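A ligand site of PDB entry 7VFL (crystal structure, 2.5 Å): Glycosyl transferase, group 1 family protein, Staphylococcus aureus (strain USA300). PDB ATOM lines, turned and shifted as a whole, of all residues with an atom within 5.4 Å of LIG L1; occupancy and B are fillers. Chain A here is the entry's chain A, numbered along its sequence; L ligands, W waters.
The side-chain hydroxyl (OG) of Ser 410 lies within hydrogen-bond range of the backbone NH (N) of Leu 413. OH of Tyr 394 is in hydrogen-bond range of OE2 of Glu 415. The backbone NH (N) of Ala 329 lies within hydrogen-bond range of the backbone carbonyl oxygen (O) of Tyr 359 (2.9 Å). The side-chain amino group of Lys 335 lies within salt-bridge range of the side-chain carboxylate of Glu 407 (2.6 Å). O of Gly 385 lies within hydrogen-bond range of N of Gly 360, at 3.0 Å. O of Gly 360 lies within hydrogen-bond range of N of Phe 386 (3.2 Å).
Water W1 lies within hydrogen-bond range of an oxygen (O12) of LIG L1 and the backbone NH of Arg 330.
Residues that only touch LIG L1: Leu 14 (3.8 Å), Gly 16 (3.4 Å), Lys 19 (3.7 Å), Val 328 (3.9 Å), Tyr 359 (3.3 Å), Gly 360 (3.8 Å), Gly 385 (3.7 Å), Phe 386 (3.5 Å), Leu 390 (3.9 Å), Glu 407 (3.9 Å) and Ser 410 (3.8 Å). Hydrophobic or aromatic side chains within 4 Å of LIG L1: Val 328, Tyr 359, Phe 386, Leu 390, Leu 411 and Ala 412. Of the 23 residues printed, 17 come within 4 Å of LIG L1. Along chain A the residues within 4 Å of LIG L1 span positions 14 to 415. The nearest printed residue that does not touch LIG L1 is Ser 388 (4.5 Å).
N of Leu 411 sits at hydrogen-bond distance from O7 of LIG L1. The backbone NH (N) of Ser 410 is in hydrogen-bond range of an oxygen (O2) of LG2 L2, 3.1 Å away. The backbone NH (N) of Ala 412 lies within hydrogen-bond range of an oxygen (O8) of LIG L1, 3.0 Å away. NZ of Lys 335 lies within salt-bridge range of O10 of LIG L1 (2.9 Å). An oxygen (O3) of LIG L1 lies within hydrogen-bond range of the side-chain carboxylate (OE1) of Glu 415, at 2.6 Å. N2 of LIG L1 lies within hydrogen-bond range of O of Leu 387 (2.7 Å). The backbone NH (N) of Leu 387 sits at hydrogen-bond distance from an oxygen (O2) of LIG L1 (3.1 Å). The guanidinium group (NE) of Arg 330 lies within salt-bridge range of an oxygen (O12) of LIG L1, at 2.8 Å. The side-chain carboxylate (OE1) of Glu 407 lies within hydrogen-bond range of an oxygen (O2) of LG2 L2, at 2.9 Å.
An oxygen (O3) of LG2 L2 sits at hydrogen-bond distance from an oxygen (O7) of LIG L1 (2.8 Å).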
ATOM      1  N   LEU A  14      -8.576  10.257  16.771  1.00  0.00           N
ATOM      2  CA  LEU A  14      -8.421  11.578  16.211  1.00  0.00           C
ATOM      3  C   LEU A  14      -9.079  11.667  14.831  1.00  0.00           C
ATOM      4  O   LEU A  14      -8.752  10.911  13.910  1.00  0.00           O
ATOM      5  CB  LEU A  14      -6.951  11.943  16.131  1.00  0.00           C
ATOM      6  CG  LEU A  14      -6.701  13.450  16.155  1.00  0.00           C
ATOM      7  CD1 LEU A  14      -7.424  14.142  17.291  1.00  0.00           C
ATOM      8  CD2 LEU A  14      -5.211  13.774  16.264  1.00  0.00           C
ATOM      9  N   THR A  15      -9.963  12.630  14.688  1.00  0.00           N
ATOM     10  CA  THR A  15     -10.615  12.935  13.436  1.00  0.00           C
ATOM     11  C   THR A  15      -9.867  13.996  12.634  1.00  0.00           C
ATOM     12  O   THR A  15      -8.932  14.650  13.118  1.00  0.00           O
ATOM     13  CB  THR A  15     -12.026  13.424  13.721  1.00  0.00           C
ATOM     14  OG1 THR A  15     -11.975  14.759  14.235  1.00  0.00           O
ATOM     15  CG2 THR A  15     -12.671  12.586  14.799  1.00  0.00           C
ATOM     16  N   GLY A  16     -10.331  14.204  11.416  1.00  0.00           N
ATOM     17  CA  GLY A  16      -9.792  15.214  10.527  1.00  0.00           C
ATOM     18  C   GLY A  16      -9.725  16.598  11.116  1.00  0.00           C
ATOM     19  O   GLY A  16      -8.651  17.174  11.222  1.00  0.00           O
ATOM     20  N   ILE A  17     -10.873  17.140  11.493  1.00  0.00           N
ATOM     21  CA  ILE A  17     -10.943  18.481  12.010  1.00  0.00           C
ATOM     22  C   ILE A  17     -10.084  18.641  13.259  1.00  0.00           C
ATOM     23  O   ILE A  17      -9.420  19.665  13.454  1.00  0.00           O
ATOM     24  CB  ILE A  17     -12.401  18.852  12.277  1.00  0.00           C
ATOM     25  CG1 ILE A  17     -13.193  18.921  10.964  1.00  0.00           C
ATOM     26  CG2 ILE A  17     -12.454  20.184  13.016  1.00  0.00           C
ATOM     27  CD1 ILE A  17     -14.551  19.690  11.089  1.00  0.00           C
ATOM     28  N   LYS A  19      -7.402  16.778  14.019  1.00  0.00           N
ATOM     29  CA  LYS A  19      -6.020  16.796  13.550  1.00  0.00           C
ATOM     30  C   LYS A  19      -5.674  18.121  12.868  1.00  0.00           C
ATOM     31  O   LYS A  19      -4.564  18.644  13.024  1.00  0.00           O
ATOM     32  CB  LYS A  19      -5.786  15.604  12.625  1.00  0.00           C
ATOM     33  CG  LYS A  19      -4.398  15.521  11.957  1.00  0.00           C
ATOM     34  CD  LYS A  19      -3.396  14.697  12.781  1.00  0.00           C
ATOM     35  CE  LYS A  19      -2.068  14.440  12.018  1.00  0.00           C
ATOM     36  NZ  LYS A  19      -2.193  13.466  10.864  1.00  0.00           N
ATOM     37  N   VAL A 328      -7.251   4.719   3.651  1.00  0.00           N
ATOM     38  CA  VAL A 328      -7.139   5.378   4.954  1.00  0.00           C
ATOM     39  C   VAL A 328      -8.301   6.354   5.004  1.00  0.00           C
ATOM     40  O   VAL A 328      -8.212   7.489   4.549  1.00  0.00           O
ATOM     41  CB  VAL A 328      -5.785   6.063   5.108  1.00  0.00           C
ATOM     42  CG1 VAL A 328      -5.707   6.893   6.351  1.00  0.00           C
ATOM     43  CG2 VAL A 328      -4.670   5.019   5.122  1.00  0.00           C
ATOM     44  N   ALA A 329      -9.406   5.909   5.603  1.00  0.00           N
ATOM     45  CA  ALA A 329     -10.642   6.673   5.541  1.00  0.00           C
ATOM     46  C   ALA A 329     -11.682   6.086   6.462  1.00  0.00           C
ATOM     47  O   ALA A 329     -11.743   4.880   6.657  1.00  0.00           O
ATOM     48  CB  ALA A 329     -11.228   6.677   4.139  1.00  0.00           C
ATOM     49  N   ARG A 330     -12.520   6.974   7.000  1.00  0.00           N
ATOM     50  CA  ARG A 330     -13.652   6.582   7.822  1.00  0.00           C
ATOM     51  C   ARG A 330     -14.555   5.587   7.077  1.00  0.00           C
ATOM     52  O   ARG A 330     -14.683   5.626   5.853  1.00  0.00           O
ATOM     53  CB  ARG A 330     -14.462   7.822   8.228  1.00  0.00           C
ATOM     54  CG  ARG A 330     -13.864   8.589   9.432  1.00  0.00           C
ATOM     55  CD  ARG A 330     -14.574   9.902   9.645  1.00  0.00           C
ATOM     56  NE  ARG A 330     -14.520  10.721   8.431  1.00  0.00           N
ATOM     57  CZ  ARG A 330     -15.575  11.030   7.686  1.00  0.00           C
ATOM     58  NH1 ARG A 330     -16.776  10.559   7.966  1.00  0.00           N
ATOM     59  NH2 ARG A 330     -15.415  11.848   6.653  1.00  0.00           N
ATOM     60  N   LYS A 335     -17.129   8.255   1.595  1.00  0.00           N
ATOM     61  CA  LYS A 335     -15.887   7.650   1.121  1.00  0.00           C
ATOM     62  C   LYS A 335     -16.125   6.515   0.123  1.00  0.00           C
ATOM     63  O   LYS A 335     -15.191   6.120  -0.583  1.00  0.00           O
ATOM     64  CB  LYS A 335     -15.089   7.117   2.319  1.00  0.00           C
ATOM     65  CG  LYS A 335     -14.859   8.098   3.449  1.00  0.00           C
ATOM     66  CD  LYS A 335     -14.074   9.347   3.002  1.00  0.00           C
ATOM     67  CE  LYS A 335     -13.447  10.058   4.228  1.00  0.00           C
ATOM     68  NZ  LYS A 335     -12.759  11.315   3.830  1.00  0.00           N
ATOM     69  N   TYR A 359      -8.037   1.249   6.759  1.00  0.00           N
ATOM     70  CA  TYR A 359      -7.908   1.801   8.096  1.00  0.00           C
ATOM     71  C   TYR A 359      -8.957   2.891   8.354  1.00  0.00           C
ATOM     72  O   TYR A 359      -9.019   3.909   7.653  1.00  0.00           O
ATOM     73  CB  TYR A 359      -6.507   2.366   8.298  1.00  0.00           C
ATOM     74  CG  TYR A 359      -5.404   1.425   7.845  1.00  0.00           C
ATOM     75  CD1 TYR A 359      -4.928   1.436   6.557  1.00  0.00           C
ATOM     76  CD2 TYR A 359      -4.841   0.525   8.705  1.00  0.00           C
ATOM     77  CE1 TYR A 359      -3.912   0.567   6.136  1.00  0.00           C
ATOM     78  CE2 TYR A 359      -3.856  -0.344   8.299  1.00  0.00           C
ATOM     79  CZ  TYR A 359      -3.368  -0.283   7.024  1.00  0.00           C
ATOM     80  OH  TYR A 359      -2.397  -1.133   6.589  1.00  0.00           O
ATOM     81  N   GLY A 360      -9.762   2.662   9.372  1.00  0.00           N
ATOM     82  CA  GLY A 360     -10.705   3.657   9.824  1.00  0.00           C
ATOM     83  C   GLY A 360     -11.732   3.009  10.734  1.00  0.00           C
ATOM     84  O   GLY A 360     -11.514   1.922  11.266  1.00  0.00           O
ATOM     85  N   GLY A 385      -9.613  -1.523  11.197  1.00  0.00           N
ATOM     86  CA  GLY A 385      -9.947  -0.653  12.288  1.00  0.00           C
ATOM     87  C   GLY A 385      -9.100   0.610  12.301  1.00  0.00           C
ATOM     88  O   GLY A 385      -8.362   0.890  11.382  1.00  0.00           O
ATOM     89  N   PHE A 386      -9.208   1.361  13.386  1.00  0.00           N
ATOM     90  CA  PHE A 386      -8.487   2.612  13.537  1.00  0.00           C
ATOM     91  C   PHE A 386      -7.185   2.339  14.260  1.00  0.00           C
ATOM     92  O   PHE A 386      -7.204   1.800  15.371  1.00  0.00           O
ATOM     93  CB  PHE A 386      -9.341   3.630  14.278  1.00  0.00           C
ATOM     94  CG  PHE A 386      -8.761   5.008  14.308  1.00  0.00           C
ATOM     95  CD1 PHE A 386      -7.840   5.363  15.271  1.00  0.00           C
ATOM     96  CD2 PHE A 386      -9.176   5.966  13.396  1.00  0.00           C
ATOM     97  CE1 PHE A 386      -7.303   6.659  15.320  1.00  0.00           C
ATOM     98  CE2 PHE A 386      -8.665   7.273  13.469  1.00  0.00           C
ATOM     99  CZ  PHE A 386      -7.710   7.602  14.450  1.00  0.00           C
ATOM    100  N   LEU A 387      -6.066   2.647  13.626  1.00  0.00           N
ATOM    101  CA  LEU A 387      -4.755   2.628  14.245  1.00  0.00           C
ATOM    102  C   LEU A 387      -4.305   4.064  14.445  1.00  0.00           C
ATOM    103  O   LEU A 387      -4.387   4.880  13.520  1.00  0.00           O
ATOM    104  CB  LEU A 387      -3.718   1.911  13.375  1.00  0.00           C
ATOM    105  CG  LEU A 387      -3.990   0.517  12.827  1.00  0.00           C
ATOM    106  CD1 LEU A 387      -2.737  -0.129  12.243  1.00  0.00           C
ATOM    107  CD2 LEU A 387      -4.522  -0.385  13.862  1.00  0.00           C
ATOM    108  N   SER A 388      -3.798   4.369  15.653  1.00  0.00           N
ATOM    109  CA  SER A 388      -3.374   5.733  15.970  1.00  0.00           C
ATOM    110  C   SER A 388      -2.016   6.036  15.420  1.00  0.00           C
ATOM    111  O   SER A 388      -1.705   7.202  15.240  1.00  0.00           O
ATOM    112  CB  SER A 388      -3.354   5.985  17.473  1.00  0.00           C
ATOM    113  OG  SER A 388      -2.510   5.053  18.104  1.00  0.00           O
ATOM    114  N   LEU A 390       0.064   5.021  11.969  1.00  0.00           N
ATOM    115  CA  LEU A 390       0.062   4.335  10.695  1.00  0.00           C
ATOM    116  C   LEU A 390       1.448   4.197  10.088  1.00  0.00           C
ATOM    117  O   LEU A 390       1.568   3.590   9.027  1.00  0.00           O
ATOM    118  CB  LEU A 390      -0.822   5.113   9.716  1.00  0.00           C
ATOM    119  CG  LEU A 390      -2.319   5.070   9.948  1.00  0.00           C
ATOM    120  CD1 LEU A 390      -3.056   5.993   8.913  1.00  0.00           C
ATOM    121  CD2 LEU A 390      -2.856   3.712   9.846  1.00  0.00           C
ATOM    122  N   TYR A 394       2.341   2.238   6.206  1.00  0.00           N
ATOM    123  CA  TYR A 394       2.702   2.826   4.925  1.00  0.00           C
ATOM    124  C   TYR A 394       3.992   2.239   4.391  1.00  0.00           C
ATOM    125  O   TYR A 394       4.252   2.349   3.188  1.00  0.00           O
ATOM    126  CB  TYR A 394       2.897   4.323   5.061  1.00  0.00           C
ATOM    127  CG  TYR A 394       1.667   5.175   5.317  1.00  0.00           C
ATOM    128  CD1 TYR A 394       0.678   5.272   4.392  1.00  0.00           C
ATOM    129  CD2 TYR A 394       1.515   5.901   6.482  1.00  0.00           C
ATOM    130  CE1 TYR A 394      -0.415   6.061   4.602  1.00  0.00           C
ATOM    131  CE2 TYR A 394       0.370   6.674   6.689  1.00  0.00           C
ATOM    132  CZ  TYR A 394      -0.564   6.755   5.734  1.00  0.00           C
ATOM    133  OH  TYR A 394      -1.687   7.520   5.881  1.00  0.00           O
ATOM    134  N   GLU A 407     -14.483  15.987  -0.377  1.00  0.00           N
ATOM    135  CA  GLU A 407     -13.422  16.254   0.572  1.00  0.00           C
ATOM    136  C   GLU A 407     -13.239  17.763   0.748  1.00  0.00           C
ATOM    137  O   GLU A 407     -13.625  18.572  -0.104  1.00  0.00           O
ATOM    138  CB  GLU A 407     -12.087  15.617   0.118  1.00  0.00           C
ATOM    139  CG  GLU A 407     -12.062  14.085   0.029  1.00  0.00           C
ATOM    140  CD  GLU A 407     -12.024  13.376   1.381  1.00  0.00           C
ATOM    141  OE1 GLU A 407     -11.651  13.969   2.401  1.00  0.00           O
ATOM    142  OE2 GLU A 407     -12.438  12.204   1.426  1.00  0.00           O
ATOM    143  N   SER A 410      -8.290  16.297   2.352  1.00  0.00           N
ATOM    144  CA  SER A 410      -7.878  14.921   2.572  1.00  0.00           C
ATOM    145  C   SER A 410      -6.488  14.870   3.195  1.00  0.00           C
ATOM    146  O   SER A 410      -5.470  14.758   2.491  1.00  0.00           O
ATOM    147  CB  SER A 410      -7.915  14.094   1.294  1.00  0.00           C
ATOM    148  OG  SER A 410      -7.470  12.772   1.622  1.00  0.00           O
ATOM    149  N   LEU A 411      -6.459  14.845   4.533  1.00  0.00           N
ATOM    150  CA  LEU A 411      -5.185  14.690   5.237  1.00  0.00           C
ATOM    151  C   LEU A 411      -4.556  13.356   4.898  1.00  0.00           C
ATOM    152  O   LEU A 411      -3.340  13.232   4.815  1.00  0.00           O
ATOM    153  CB  LEU A 411      -5.365  14.812   6.753  1.00  0.00           C
ATOM    154  CG  LEU A 411      -5.875  16.159   7.260  1.00  0.00           C
ATOM    155  CD1 LEU A 411      -6.471  16.048   8.617  1.00  0.00           C
ATOM    156  CD2 LEU A 411      -4.738  17.127   7.321  1.00  0.00           C
ATOM    157  N   ALA A 412      -5.370  12.324   4.749  1.00  0.00           N
ATOM    158  CA  ALA A 412      -4.836  11.016   4.398  1.00  0.00           C
ATOM    159  C   ALA A 412      -4.143  10.988   3.030  1.00  0.00           C
ATOM    160  O   ALA A 412      -3.180  10.239   2.843  1.00  0.00           O
ATOM    161  CB  ALA A 412      -5.985  10.033   4.459  1.00  0.00           C
ATOM    162  N   LEU A 413      -4.627  11.770   2.067  1.00  0.00           N
ATOM    163  CA  LEU A 413      -3.933  11.866   0.780  1.00  0.00           C
ATOM    164  C   LEU A 413      -2.521  12.414   0.925  1.00  0.00           C
ATOM    165  O   LEU A 413      -1.573  11.818   0.426  1.00  0.00           O
ATOM    166  CB  LEU A 413      -4.737  12.729  -0.180  1.00  0.00           C
ATOM    167  CG  LEU A 413      -4.499  12.420  -1.651  1.00  0.00           C
ATOM    168  CD1 LEU A 413      -5.618  13.081  -2.532  1.00  0.00           C
ATOM    169  CD2 LEU A 413      -3.078  12.927  -2.061  1.00  0.00           C
ATOM    170  N   GLU A 415      -0.666  12.651   3.681  1.00  0.00           N
ATOM    171  CA  GLU A 415       0.065  11.712   4.532  1.00  0.00           C
ATOM    172  C   GLU A 415       0.598  10.521   3.751  1.00  0.00           C
ATOM    173  O   GLU A 415       1.723  10.045   3.990  1.00  0.00           O
ATOM    174  CB  GLU A 415      -0.870  11.250   5.629  1.00  0.00           C
ATOM    175  CG  GLU A 415      -0.297  10.778   6.931  1.00  0.00           C
ATOM    176  CD  GLU A 415      -1.406  10.151   7.830  1.00  0.00           C
ATOM    177  OE1 GLU A 415      -2.602  10.599   7.723  1.00  0.00           O
ATOM    178  OE2 GLU A 415      -1.039   9.213   8.616  1.00  0.00           O
HETATM  179  N1  LIG L   1      -6.554   8.131  10.604  1.00  0.00           N
HETATM  180  C1  LIG L   1      -5.745   7.465  11.546  1.00  0.00           C
HETATM  181  N2  LIG L   1      -5.811   6.144  11.664  1.00  0.00           N
HETATM  182  C2  LIG L   1      -6.637   5.429  10.916  1.00  0.00           C
HETATM  183  C3  LIG L   1      -7.440   6.054   9.987  1.00  0.00           C
HETATM  184  C4  LIG L   1      -7.388   7.432   9.839  1.00  0.00           C
HETATM  185  O1  LIG L   1      -4.968   8.114  12.273  1.00  0.00           O
HETATM  186  O2  LIG L   1      -6.674   4.200  11.055  1.00  0.00           O
HETATM  187  C5  LIG L   1      -6.464   9.586  10.494  1.00  0.00           C
HETATM  188  C6  LIG L   1      -5.677   9.968   9.262  1.00  0.00           C
HETATM  189  O3  LIG L   1      -4.293  10.021   9.581  1.00  0.00           O
HETATM  190  C7  LIG L   1      -6.248  11.311   8.872  1.00  0.00           C
HETATM  191  C8  LIG L   1      -7.604  11.380   9.530  1.00  0.00           C
HETATM  192  O4  LIG L   1      -7.735  10.197  10.322  1.00  0.00           O
HETATM  193  O5  LIG L   1      -5.434  12.376   9.339  1.00  0.00           O
HETATM  194  C9  LIG L   1      -8.718  11.441   8.506  1.00  0.00           C
HETATM  195  O6  LIG L   1      -8.765  12.757   7.954  1.00  0.00           O
HETATM  196  P1  LIG L   1      -9.082  13.027   6.415  1.00  0.00           P
HETATM  197  O7  LIG L   1      -8.984  14.481   6.133  1.00  0.00           O
HETATM  198  O8  LIG L   1      -8.261  12.086   5.602  1.00  0.00           O
HETATM  199  O9  LIG L   1     -10.596  12.564   6.257  1.00  0.00           O
HETATM  200  P2  LIG L   1     -11.835  13.139   7.083  1.00  0.00           P
HETATM  201  O10 LIG L   1     -12.870  13.262   6.025  1.00  0.00           O
HETATM  202  O11 LIG L   1     -11.398  14.421   7.696  1.00  0.00           O
HETATM  203  O12 LIG L   1     -12.100  12.108   8.130  1.00  0.00           O
HETATM  204  C1  LG2 L   2     -12.949  16.994   6.826  1.00  0.00           C
HETATM  205  C2  LG2 L   2     -12.762  16.800   5.315  1.00  0.00           C
HETATM  206  C3  LG2 L   2     -11.293  16.525   5.015  1.00  0.00           C
HETATM  207  C4  LG2 L   2     -10.396  17.567   5.654  1.00  0.00           C
HETATM  208  C5  LG2 L   2     -10.709  17.676   7.143  1.00  0.00           C
HETATM  209  C6  LG2 L   2      -9.822  18.716   7.802  1.00  0.00           C
HETATM  210  C7  LG2 L   2     -14.728  15.826   4.239  1.00  0.00           C
HETATM  211  C8  LG2 L   2     -15.564  14.584   4.194  1.00  0.00           C
HETATM  212  N1  LG2 L   2     -13.546  15.691   4.817  1.00  0.00           N
HETATM  213  O1  LG2 L   2     -14.296  17.344   7.139  1.00  0.00           O
HETATM  214  O2  LG2 L   2     -11.096  16.551   3.601  1.00  0.00           O
HETATM  215  O3  LG2 L   2      -9.040  17.162   5.493  1.00  0.00           O
HETATM  216  O4  LG2 L   2     -12.078  18.030   7.292  1.00  0.00           O
HETATM  217  O5  LG2 L   2      -9.887  19.929   7.054  1.00  0.00           O
HETATM  218  O6  LG2 L   2     -15.112  16.868   3.761  1.00  0.00           O
HETATM  219  O   HOH W   1     -11.421   9.843   7.065  1.00  0.00           O
